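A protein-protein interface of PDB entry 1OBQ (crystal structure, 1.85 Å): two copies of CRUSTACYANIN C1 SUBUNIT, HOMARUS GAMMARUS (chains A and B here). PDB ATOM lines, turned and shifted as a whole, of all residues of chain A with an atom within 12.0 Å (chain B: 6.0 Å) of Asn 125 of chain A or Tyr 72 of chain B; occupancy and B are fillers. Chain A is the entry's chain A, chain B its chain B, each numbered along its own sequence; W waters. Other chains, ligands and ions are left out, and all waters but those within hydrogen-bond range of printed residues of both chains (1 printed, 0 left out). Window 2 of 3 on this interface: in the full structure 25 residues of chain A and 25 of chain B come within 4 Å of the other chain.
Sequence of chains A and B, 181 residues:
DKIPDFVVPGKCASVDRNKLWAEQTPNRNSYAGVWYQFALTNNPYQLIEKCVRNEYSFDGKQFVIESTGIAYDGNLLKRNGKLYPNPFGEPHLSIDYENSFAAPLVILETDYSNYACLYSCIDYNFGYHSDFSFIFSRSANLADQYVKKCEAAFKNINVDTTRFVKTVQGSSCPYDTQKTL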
ATOM      1  N   VAL A   7     -16.448   7.616 -15.384  1.00  0.00           N
ATOM      2  CA  VAL A   7     -16.309   9.038 -15.606  1.00  0.00           C
ATOM      3  C   VAL A   7     -17.306   9.684 -14.595  1.00  0.00           C
ATOM      4  O   VAL A   7     -18.520   9.401 -14.682  1.00  0.00           O
ATOM      5  CB  VAL A   7     -16.626   9.347 -17.017  1.00  0.00           C
ATOM      6  CG1 VAL A   7     -16.500  10.832 -17.271  1.00  0.00           C
ATOM      7  CG2 VAL A   7     -15.724   8.526 -17.958  1.00  0.00           C
ATOM      8  N   VAL A   8     -16.791  10.392 -13.593  1.00  0.00           N
ATOM      9  CA  VAL A   8     -17.551  10.822 -12.455  1.00  0.00           C
ATOM     10  C   VAL A   8     -17.429  12.290 -12.221  1.00  0.00           C
ATOM     11  O   VAL A   8     -16.321  12.843 -12.306  1.00  0.00           O
ATOM     12  CB  VAL A   8     -16.992  10.114 -11.180  1.00  0.00           C
ATOM     13  CG1 VAL A   8     -17.793  10.445  -9.924  1.00  0.00           C
ATOM     14  CG2 VAL A   8     -16.905   8.607 -11.404  1.00  0.00           C
ATOM     15  N   PRO A   9     -18.557  12.989 -11.971  1.00  0.00           N
ATOM     16  CA  PRO A   9     -18.497  14.438 -11.785  1.00  0.00           C
ATOM     17  C   PRO A   9     -17.630  14.841 -10.677  1.00  0.00           C
ATOM     18  O   PRO A   9     -17.496  14.130  -9.684  1.00  0.00           O
ATOM     19  CB  PRO A   9     -20.004  14.803 -11.542  1.00  0.00           C
ATOM     20  CG  PRO A   9     -20.715  13.733 -12.115  1.00  0.00           C
ATOM     21  CD  PRO A   9     -19.960  12.514 -11.919  1.00  0.00           C
ATOM     22  N   GLY A  10     -16.931  15.955 -10.821  1.00  0.00           N
ATOM     23  CA  GLY A  10     -16.150  16.395  -9.701  1.00  0.00           C
ATOM     24  C   GLY A  10     -14.676  16.154  -9.910  1.00  0.00           C
ATOM     25  O   GLY A  10     -14.297  15.585 -10.887  1.00  0.00           O
ATOM     26  N   LYS A  11     -13.878  16.553  -8.947  1.00  0.00           N
ATOM     27  CA  LYS A  11     -12.439  16.439  -9.013  1.00  0.00           C
ATOM     28  C   LYS A  11     -11.981  15.170  -8.281  1.00  0.00           C
ATOM     29  O   LYS A  11     -12.689  14.675  -7.458  1.00  0.00           O
ATOM     30  CB  LYS A  11     -11.804  17.700  -8.372  1.00  0.00           C
ATOM     31  CG  LYS A  11     -12.014  18.927  -9.234  1.00  0.00           C
ATOM     32  CD  LYS A  11     -11.283  20.120  -8.664  1.00  0.00           C
ATOM     33  CE  LYS A  11     -11.680  21.375  -9.436  1.00  0.00           C
ATOM     34  NZ  LYS A  11     -10.643  22.424  -9.254  1.00  0.00           N
ATOM     35  N   CYS A  12     -10.829  14.636  -8.646  1.00  0.00           N
ATOM     36  CA  CYS A  12     -10.270  13.522  -7.866  1.00  0.00           C
ATOM     37  C   CYS A  12     -10.268  13.870  -6.354  1.00  0.00           C
ATOM     38  O   CYS A  12      -9.955  14.979  -5.942  1.00  0.00           O
ATOM     39  CB  CYS A  12      -8.844  13.233  -8.312  1.00  0.00           C
ATOM     40  SG  CYS A  12      -8.761  12.493  -9.925  1.00  0.00           S
ATOM     41  N   CYS A 121      -6.345   7.929  -9.986  1.00  0.00           N
ATOM     42  CA  CYS A 121      -7.362   8.920 -10.433  1.00  0.00           C
ATOM     43  C   CYS A 121      -6.756   9.936 -11.369  1.00  0.00           C
ATOM     44  O   CYS A 121      -5.589  10.402 -11.114  1.00  0.00           O
ATOM     45  CB  CYS A 121      -7.930   9.662  -9.251  1.00  0.00           C
ATOM     46  SG  CYS A 121      -9.458  10.606  -9.544  1.00  0.00           S
ATOM     47  N   ILE A 122      -7.549  10.330 -12.379  1.00  0.00           N
ATOM     48  CA  ILE A 122      -7.165  11.344 -13.356  1.00  0.00           C
ATOM     49  C   ILE A 122      -8.301  12.407 -13.551  1.00  0.00           C
ATOM     50  O   ILE A 122      -9.485  12.030 -13.661  1.00  0.00           O
ATOM     51  CB  ILE A 122      -6.824  10.670 -14.661  1.00  0.00           C
ATOM     52  CG1 ILE A 122      -6.409  11.630 -15.752  1.00  0.00           C
ATOM     53  CG2 ILE A 122      -8.009  10.071 -15.350  1.00  0.00           C
ATOM     54  CD1 ILE A 122      -5.048  12.098 -15.685  1.00  0.00           C
ATOM     55  N   ASP A 123      -7.924  13.684 -13.454  1.00  0.00           N
ATOM     56  CA  ASP A 123      -8.833  14.792 -13.746  1.00  0.00           C
ATOM     57  C   ASP A 123      -8.881  15.123 -15.205  1.00  0.00           C
ATOM     58  O   ASP A 123      -7.839  15.128 -15.880  1.00  0.00           O
ATOM     59  CB  ASP A 123      -8.418  15.956 -12.977  1.00  0.00           C
ATOM     60  CG  ASP A 123      -8.775  15.845 -11.541  1.00  0.00           C
ATOM     61  OD1 ASP A 123      -9.892  15.535 -11.126  1.00  0.00           O
ATOM     62  OD2 ASP A 123      -7.966  16.119 -10.661  1.00  0.00           O
ATOM     63  N   TYR A 124     -10.080  15.406 -15.711  1.00  0.00           N
ATOM     64  CA  TYR A 124     -10.224  15.854 -17.080  1.00  0.00           C
ATOM     65  C   TYR A 124     -10.361  17.367 -17.063  1.00  0.00           C
ATOM     66  O   TYR A 124     -10.576  17.962 -16.004  1.00  0.00           O
ATOM     67  CB  TYR A 124     -11.446  15.261 -17.703  1.00  0.00           C
ATOM     68  CG  TYR A 124     -11.429  13.776 -17.841  1.00  0.00           C
ATOM     69  CD1 TYR A 124     -10.480  13.148 -18.657  1.00  0.00           C
ATOM     70  CD2 TYR A 124     -12.337  12.971 -17.176  1.00  0.00           C
ATOM     71  CE1 TYR A 124     -10.457  11.730 -18.797  1.00  0.00           C
ATOM     72  CE2 TYR A 124     -12.286  11.543 -17.283  1.00  0.00           C
ATOM     73  CZ  TYR A 124     -11.396  10.936 -18.151  1.00  0.00           C
ATOM     74  OH  TYR A 124     -11.286   9.544 -18.257  1.00  0.00           O
ATOM     75  N   ASN A 125     -10.255  17.968 -18.247  1.00  0.00           N
ATOM     76  CA  ASN A 125     -10.432  19.388 -18.354  1.00  0.00           C
ATOM     77  C   ASN A 125     -11.866  19.849 -18.253  1.00  0.00           C
ATOM     78  O   ASN A 125     -12.126  21.103 -18.213  1.00  0.00           O
ATOM     79  CB  ASN A 125      -9.752  19.985 -19.612  1.00  0.00           C
ATOM     80  CG  ASN A 125     -10.260  19.427 -20.894  1.00  0.00           C
ATOM     81  OD1 ASN A 125     -11.365  18.885 -20.939  1.00  0.00           O
ATOM     82  ND2 ASN A 125      -9.500  19.657 -22.010  1.00  0.00           N
ATOM     83  N   PHE A 126     -12.822  18.921 -18.214  1.00  0.00           N
ATOM     84  CA  PHE A 126     -14.286  19.330 -18.292  1.00  0.00           C
ATOM     85  C   PHE A 126     -15.132  19.053 -16.982  1.00  0.00           C
ATOM     86  O   PHE A 126     -16.294  18.757 -17.085  1.00  0.00           O
ATOM     87  CB  PHE A 126     -14.900  18.733 -19.542  1.00  0.00           C
ATOM     88  CG  PHE A 126     -14.914  17.206 -19.568  1.00  0.00           C
ATOM     89  CD1 PHE A 126     -15.908  16.489 -18.933  1.00  0.00           C
ATOM     90  CD2 PHE A 126     -13.941  16.479 -20.286  1.00  0.00           C
ATOM     91  CE1 PHE A 126     -15.900  15.087 -18.951  1.00  0.00           C
ATOM     92  CE2 PHE A 126     -13.935  15.132 -20.286  1.00  0.00           C
ATOM     93  CZ  PHE A 126     -14.930  14.409 -19.645  1.00  0.00           C
ATOM     94  N   GLY A 127     -14.541  19.145 -15.799  1.00  0.00           N
ATOM     95  CA  GLY A 127     -15.250  19.043 -14.502  1.00  0.00           C
ATOM     96  C   GLY A 127     -15.611  17.596 -14.036  1.00  0.00           C
ATOM     97  O   GLY A 127     -16.499  17.422 -13.182  1.00  0.00           O
ATOM     98  N   TYR A 128     -14.887  16.583 -14.597  1.00  0.00           N
ATOM     99  CA  TYR A 128     -15.084  15.191 -14.253  1.00  0.00           C
ATOM    100  C   TYR A 128     -13.686  14.556 -14.021  1.00  0.00           C
ATOM    101  O   TYR A 128     -12.650  15.160 -14.316  1.00  0.00           O
ATOM    102  CB  TYR A 128     -15.750  14.364 -15.309  1.00  0.00           C
ATOM    103  CG  TYR A 128     -17.215  14.613 -15.574  1.00  0.00           C
ATOM    104  CD1 TYR A 128     -17.646  15.821 -16.056  1.00  0.00           C
ATOM    105  CD2 TYR A 128     -18.177  13.622 -15.297  1.00  0.00           C
ATOM    106  CE1 TYR A 128     -18.982  16.018 -16.314  1.00  0.00           C
ATOM    107  CE2 TYR A 128     -19.542  13.838 -15.485  1.00  0.00           C
ATOM    108  CZ  TYR A 128     -19.924  15.059 -15.992  1.00  0.00           C
ATOM    109  OH  TYR A 128     -21.243  15.305 -16.237  1.00  0.00           O
ATOM    110  N   HIS A 129     -13.717  13.388 -13.398  1.00  0.00           N
ATOM    111  CA  HIS A 129     -12.473  12.593 -13.182  1.00  0.00           C
ATOM    112  C   HIS A 129     -12.783  11.164 -13.569  1.00  0.00           C
ATOM    113  O   HIS A 129     -13.957  10.763 -13.660  1.00  0.00           O
ATOM    114  CB  HIS A 129     -11.999  12.722 -11.792  1.00  0.00           C
ATOM    115  CG  HIS A 129     -12.894  12.155 -10.732  1.00  0.00           C
ATOM    116  ND1 HIS A 129     -14.012  12.818 -10.253  1.00  0.00           N
ATOM    117  CD2 HIS A 129     -12.795  11.008 -10.011  1.00  0.00           C
ATOM    118  CE1 HIS A 129     -14.613  12.058  -9.347  1.00  0.00           C
ATOM    119  NE2 HIS A 129     -13.896  10.961  -9.179  1.00  0.00           N
ATOM    120  N   SER A 130     -11.745  10.359 -13.767  1.00  0.00           N
ATOM    121  CA  SER A 130     -11.952   8.932 -13.884  1.00  0.00           C
ATOM    122  C   SER A 130     -11.056   8.313 -12.861  1.00  0.00           C
ATOM    123  O   SER A 130      -9.939   8.744 -12.663  1.00  0.00           O
ATOM    124  CB  SER A 130     -11.579   8.325 -15.213  1.00  0.00           C
ATOM    125  OG  SER A 130     -12.592   8.536 -16.166  1.00  0.00           O
ATOM    126  N   ASN B  43      -8.936  16.937 -26.847  1.00  0.00           N
ATOM    127  CA  ASN B  43      -8.113  16.330 -25.848  1.00  0.00           C
ATOM    128  C   ASN B  43      -8.678  16.772 -24.481  1.00  0.00           C
ATOM    129  O   ASN B  43      -8.621  17.917 -24.131  1.00  0.00           O
ATOM    130  CB  ASN B  43      -6.663  16.872 -26.030  1.00  0.00           C
ATOM    131  CG  ASN B  43      -5.648  16.189 -25.122  1.00  0.00           C
ATOM    132  OD1 ASN B  43      -5.943  15.823 -23.939  1.00  0.00           O
ATOM    133  ND2 ASN B  43      -4.421  16.002 -25.633  1.00  0.00           N
ATOM    134  N   PRO B  44      -9.185  15.822 -23.737  1.00  0.00           N
ATOM    135  CA  PRO B  44      -9.713  16.045 -22.395  1.00  0.00           C
ATOM    136  C   PRO B  44      -8.721  16.163 -21.312  1.00  0.00           C
ATOM    137  O   PRO B  44      -9.159  16.388 -20.123  1.00  0.00           O
ATOM    138  CB  PRO B  44     -10.642  14.800 -22.210  1.00  0.00           C
ATOM    139  CG  PRO B  44      -9.952  13.699 -22.908  1.00  0.00           C
ATOM    140  CD  PRO B  44      -9.251  14.412 -24.118  1.00  0.00           C
ATOM    141  N   TYR B  45      -7.417  16.038 -21.589  1.00  0.00           N
ATOM    142  CA  TYR B  45      -6.368  16.118 -20.562  1.00  0.00           C
ATOM    143  C   TYR B  45      -5.588  17.441 -20.601  1.00  0.00           C
ATOM    144  O   TYR B  45      -4.731  17.764 -19.729  1.00  0.00           O
ATOM    145  CB  TYR B  45      -5.378  14.997 -20.822  1.00  0.00           C
ATOM    146  CG  TYR B  45      -6.072  13.629 -20.902  1.00  0.00           C
ATOM    147  CD1 TYR B  45      -6.506  13.000 -19.755  1.00  0.00           C
ATOM    148  CD2 TYR B  45      -6.151  12.923 -22.087  1.00  0.00           C
ATOM    149  CE1 TYR B  45      -7.043  11.713 -19.787  1.00  0.00           C
ATOM    150  CE2 TYR B  45      -6.687  11.635 -22.164  1.00  0.00           C
ATOM    151  CZ  TYR B  45      -7.141  11.026 -21.011  1.00  0.00           C
ATOM    152  OH  TYR B  45      -7.713   9.769 -21.097  1.00  0.00           O
ATOM    153  N   GLN B  46      -5.866  18.205 -21.622  1.00  0.00           N
ATOM    154  CA  GLN B  46      -5.127  19.463 -21.897  1.00  0.00           C
ATOM    155  C   GLN B  46      -5.835  20.544 -21.091  1.00  0.00           C
ATOM    156  O   GLN B  46      -6.959  20.922 -21.418  1.00  0.00           O
ATOM    157  CB  GLN B  46      -5.121  19.820 -23.412  1.00  0.00           C
ATOM    158  CG  GLN B  46      -4.680  21.277 -23.831  1.00  0.00           C
ATOM    159  CD  GLN B  46      -3.280  21.700 -23.260  1.00  0.00           C
ATOM    160  OE1 GLN B  46      -3.140  21.838 -22.045  1.00  0.00           O
ATOM    161  NE2 GLN B  46      -2.261  21.863 -24.150  1.00  0.00           N
ATOM    162  N   LEU B  47      -5.202  21.009 -20.014  1.00  0.00           N
ATOM    163  CA  LEU B  47      -5.795  22.014 -19.126  1.00  0.00           C
ATOM    164  C   LEU B  47      -5.660  23.461 -19.622  1.00  0.00           C
ATOM    165  O   LEU B  47      -6.383  24.314 -19.172  1.00  0.00           O
ATOM    166  CB  LEU B  47      -5.200  21.885 -17.738  1.00  0.00           C
ATOM    167  CG  LEU B  47      -5.442  20.549 -17.024  1.00  0.00           C
ATOM    168  CD1 LEU B  47      -4.854  20.556 -15.625  1.00  0.00           C
ATOM    169  CD2 LEU B  47      -6.975  20.297 -16.918  1.00  0.00           C
ATOM    170  N   ILE B  48      -4.809  23.695 -20.608  1.00  0.00           N
ATOM    171  CA  ILE B  48      -4.541  25.034 -21.087  1.00  0.00           C
ATOM    172  C   ILE B  48      -5.240  25.209 -22.418  1.00  0.00           C
ATOM    173  O   ILE B  48      -5.005  24.427 -23.359  1.00  0.00           O
ATOM    174  CB  ILE B  48      -3.019  25.274 -21.248  1.00  0.00           C
ATOM    175  CG1 ILE B  48      -2.330  24.941 -19.952  1.00  0.00           C
ATOM    176  CG2 ILE B  48      -2.802  26.750 -21.645  1.00  0.00           C
ATOM    177  CD1 ILE B  48      -0.859  24.924 -20.083  1.00  0.00           C
ATOM    178  N   GLU B  49      -6.197  26.153 -22.495  1.00  0.00           N
ATOM    179  CA  GLU B  49      -7.066  26.311 -23.642  1.00  0.00           C
ATOM    180  C   GLU B  49      -6.499  27.208 -24.777  1.00  0.00           C
ATOM    181  O   GLU B  49      -6.629  26.876 -25.973  1.00  0.00           O
ATOM    182  CB  GLU B  49      -8.412  26.924 -23.224  1.00  0.00           C
ATOM    183  CG  GLU B  49      -9.344  26.918 -24.407  1.00  0.00           C
ATOM    184  CD  GLU B  49     -10.711  27.593 -24.124  1.00  0.00           C
ATOM    185  OE1 GLU B  49     -10.897  28.132 -23.051  1.00  0.00           O
ATOM    186  OE2 GLU B  49     -11.597  27.530 -24.974  1.00  0.00           O
ATOM    187  N   ILE B  70      -3.707  30.377 -21.115  1.00  0.00           N
ATOM    188  CA  ILE B  70      -4.970  30.691 -20.450  1.00  0.00           C
ATOM    189  C   ILE B  70      -5.729  29.364 -20.270  1.00  0.00           C
ATOM    190  O   ILE B  70      -5.999  28.652 -21.239  1.00  0.00           O
ATOM    191  CB  ILE B  70      -5.703  31.682 -21.246  1.00  0.00           C
ATOM    192  CG1 ILE B  70      -4.841  32.954 -21.402  1.00  0.00           C
ATOM    193  CG2 ILE B  70      -7.041  32.108 -20.588  1.00  0.00           C
ATOM    194  CD1 ILE B  70      -5.441  33.895 -22.365  1.00  0.00           C
ATOM    195  N   ALA B  71      -6.032  29.019 -19.014  1.00  0.00           N
ATOM    196  CA  ALA B  71      -6.890  27.875 -18.752  1.00  0.00           C
ATOM    197  C   ALA B  71      -8.365  28.095 -19.198  1.00  0.00           C
ATOM    198  O   ALA B  71      -8.803  29.178 -19.486  1.00  0.00           O
ATOM    199  CB  ALA B  71      -6.830  27.529 -17.281  1.00  0.00           C
ATOM    200  N   TYR B  72      -9.149  27.003 -19.145  1.00  0.00           N
ATOM    201  CA  TYR B  72     -10.520  27.042 -19.512  1.00  0.00           C
ATOM    202  C   TYR B  72     -11.355  27.981 -18.624  1.00  0.00           C
ATOM    203  O   TYR B  72     -12.393  28.425 -19.067  1.00  0.00           O
ATOM    204  CB  TYR B  72     -11.107  25.662 -19.457  1.00  0.00           C
ATOM    205  CG  TYR B  72     -10.753  24.879 -20.672  1.00  0.00           C
ATOM    206  CD1 TYR B  72     -11.507  24.972 -21.794  1.00  0.00           C
ATOM    207  CD2 TYR B  72      -9.612  24.090 -20.680  1.00  0.00           C
ATOM    208  CE1 TYR B  72     -11.150  24.254 -22.961  1.00  0.00           C
ATOM    209  CE2 TYR B  72      -9.263  23.349 -21.787  1.00  0.00           C
ATOM    210  CZ  TYR B  72     -10.027  23.449 -22.933  1.00  0.00           C
ATOM    211  OH  TYR B  72      -9.666  22.752 -24.048  1.00  0.00           O
ATOM    212  N   ASP B  73     -10.913  28.244 -17.401  1.00  0.00           N
ATOM    213  CA  ASP B  73     -11.566  29.268 -16.572  1.00  0.00           C
ATOM    214  C   ASP B  73     -11.114  30.724 -16.826  1.00  0.00           C
ATOM    215  O   ASP B  73     -11.624  31.643 -16.195  1.00  0.00           O
ATOM    216  CB  ASP B  73     -11.449  28.953 -15.112  1.00  0.00           C
ATOM    217  CG  ASP B  73     -10.046  29.023 -14.606  1.00  0.00           C
ATOM    218  OD1 ASP B  73      -9.071  29.471 -15.298  1.00  0.00           O
ATOM    219  OD2 ASP B  73      -9.862  28.597 -13.481  1.00  0.00           O
ATOM    220  N   GLY B  74     -10.178  30.959 -17.746  1.00  0.00           N
ATOM    221  CA  GLY B  74      -9.817  32.322 -18.045  1.00  0.00           C
ATOM    222  C   GLY B  74      -8.617  32.748 -17.277  1.00  0.00           C
ATOM    223  O   GLY B  74      -8.066  33.821 -17.532  1.00  0.00           O
ATOM    224  N   ASN B  75      -8.174  31.927 -16.360  1.00  0.00           N
ATOM    225  CA  ASN B  75      -6.978  32.261 -15.660  1.00  0.00           C
ATOM    226  C   ASN B  75      -5.649  31.793 -16.314  1.00  0.00           C
ATOM    227  O   ASN B  75      -5.631  30.790 -17.053  1.00  0.00           O
ATOM    228  CB  ASN B  75      -7.074  31.739 -14.285  1.00  0.00           C
ATOM    229  CG  ASN B  75      -8.064  32.603 -13.444  1.00  0.00           C
ATOM    230  OD1 ASN B  75      -7.826  33.812 -13.247  1.00  0.00           O
ATOM    231  ND2 ASN B  75      -9.227  32.057 -13.159  1.00  0.00           N
HETATM  232  O   HOH W   1      -8.875   8.190 -19.006  1.00  0.00           O
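No position is printed for both chains. Of the 8 pairs that touch across the chains among the printed residues, none has its exchanged pair printed and touching as well.
Among the printed residues, merely in contact across the chains: Tyr 124 of chain A with Pro 44 of chain B, Tyr 124 of chain A with Tyr 45 of chain B, Asn 125 of chain A with Tyr 72 of chain B, Phe 126 of chain A with Pro 44 of chain B and Asn 125 of chain A with Leu 47 of chain B.
Water W1 bridges the side-chain hydroxyl (OH) of Tyr 124 of chain A (2.9 Å) and the side-chain hydroxyl (OH) of Tyr 45 of chain B (2.9 Å).
Of the printed residues of chain B, Tyr 124 of chain A touches Pro 44 and Tyr 45. Of chain B, only Asn 43, Pro 44, Gln 46, Leu 47 and Tyr 72 come within 4 Å of Asn 125 of chain A. Of the printed residues of chain B, Phe 126 of chain A touches Pro 44. Asn 43 of chain B touches just one residue of chain A: Asn 125. Pro 44 of chain B touches just these residues of chain A: Tyr 124 (3.3 Å), Asn 125 (2.7 Å) and Phe 126 (3.8 Å). Of the printed residues of chain A, Tyr 45 of chain B touches Tyr 124. Gln 46 of chain B touches just one residue of chain A: Asn 125 (2.9 Å). Of chain A, only Asn 125 (3.9 Å) comes within 4 Å of Leu 47 of chain B. No residue of chain A comes within 4 Å of Glu 49 of chain B. Of chain A, only Asn 125 (3.7 Å) comes within 4 Å of Tyr 72 of chain B. No residue of chain A comes within 4 Å of Asp 73 of chain B. The nearest residue of chain A that does not touch Tyr 72 of chain B is Phe 126 of chain A (6.6 Å).
Of the 16 printed residues of chain A, 3 touch a printed residue of chain B. Hydrophobic or aromatic side chains of chain A that line the printed part of chain B: Tyr 124 and Phe 126. Along chain A the printed residues that touch a printed residue of chain B span positions 124 to 126. Of the 13 printed residues of chain B, 6 touch a printed residue of chain A. Printed residues of chain B that touch a printed residue of chain A: Asn 43, Pro 44, Tyr 45, Gln 46, Leu 47 and Tyr 72. Hydrophobic or aromatic side chains of chain B within 4 Å of the printed part of chain A: Pro 44, Tyr 45, Leu 47 and Tyr 72. Among the printed residues, 8 pairs touch across the chains.
The side-chain amide nitrogen (ND2) of Asn 125 of chain A sits at hydrogen-bond distance from the backbone carbonyl oxygen (O) of Asn 43 of chain B (2.9 Å). O of Pro 44 of chain B sits at hydrogen-bond distance from N of Asn 125 of chain A, 2.7 Å away. O of Gln 46 of chain B lies within hydrogen-bond range of ND2 of Asn 125 of chain A (2.9 Å).
The side-chain hydroxyl (OG) of Ser 130 of chain A lies within hydrogen-bond range of the side-chain hydroxyl (OH) of Tyr 124 of chain A (2.7 Å). The side-chain sulfur of Cys 12 of chain A is disulfide-bonded to the side-chain sulfur of Cys 121 of chain A (2.0 Å). N of Gln 46 of chain B is in hydrogen-bond range of OD1 of Asn 43 of chain B, 3.3 Å away. The side-chain amide oxygen of Asn 43 of chain B lies within hydrogen-bond range of the backbone NH of Tyr 45 of chain B (2.8 Å). The backbone NH of Ile 48 of chain B is in hydrogen-bond range of the side-chain amide oxygen of Gln 46 of chain B (2.9 Å).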
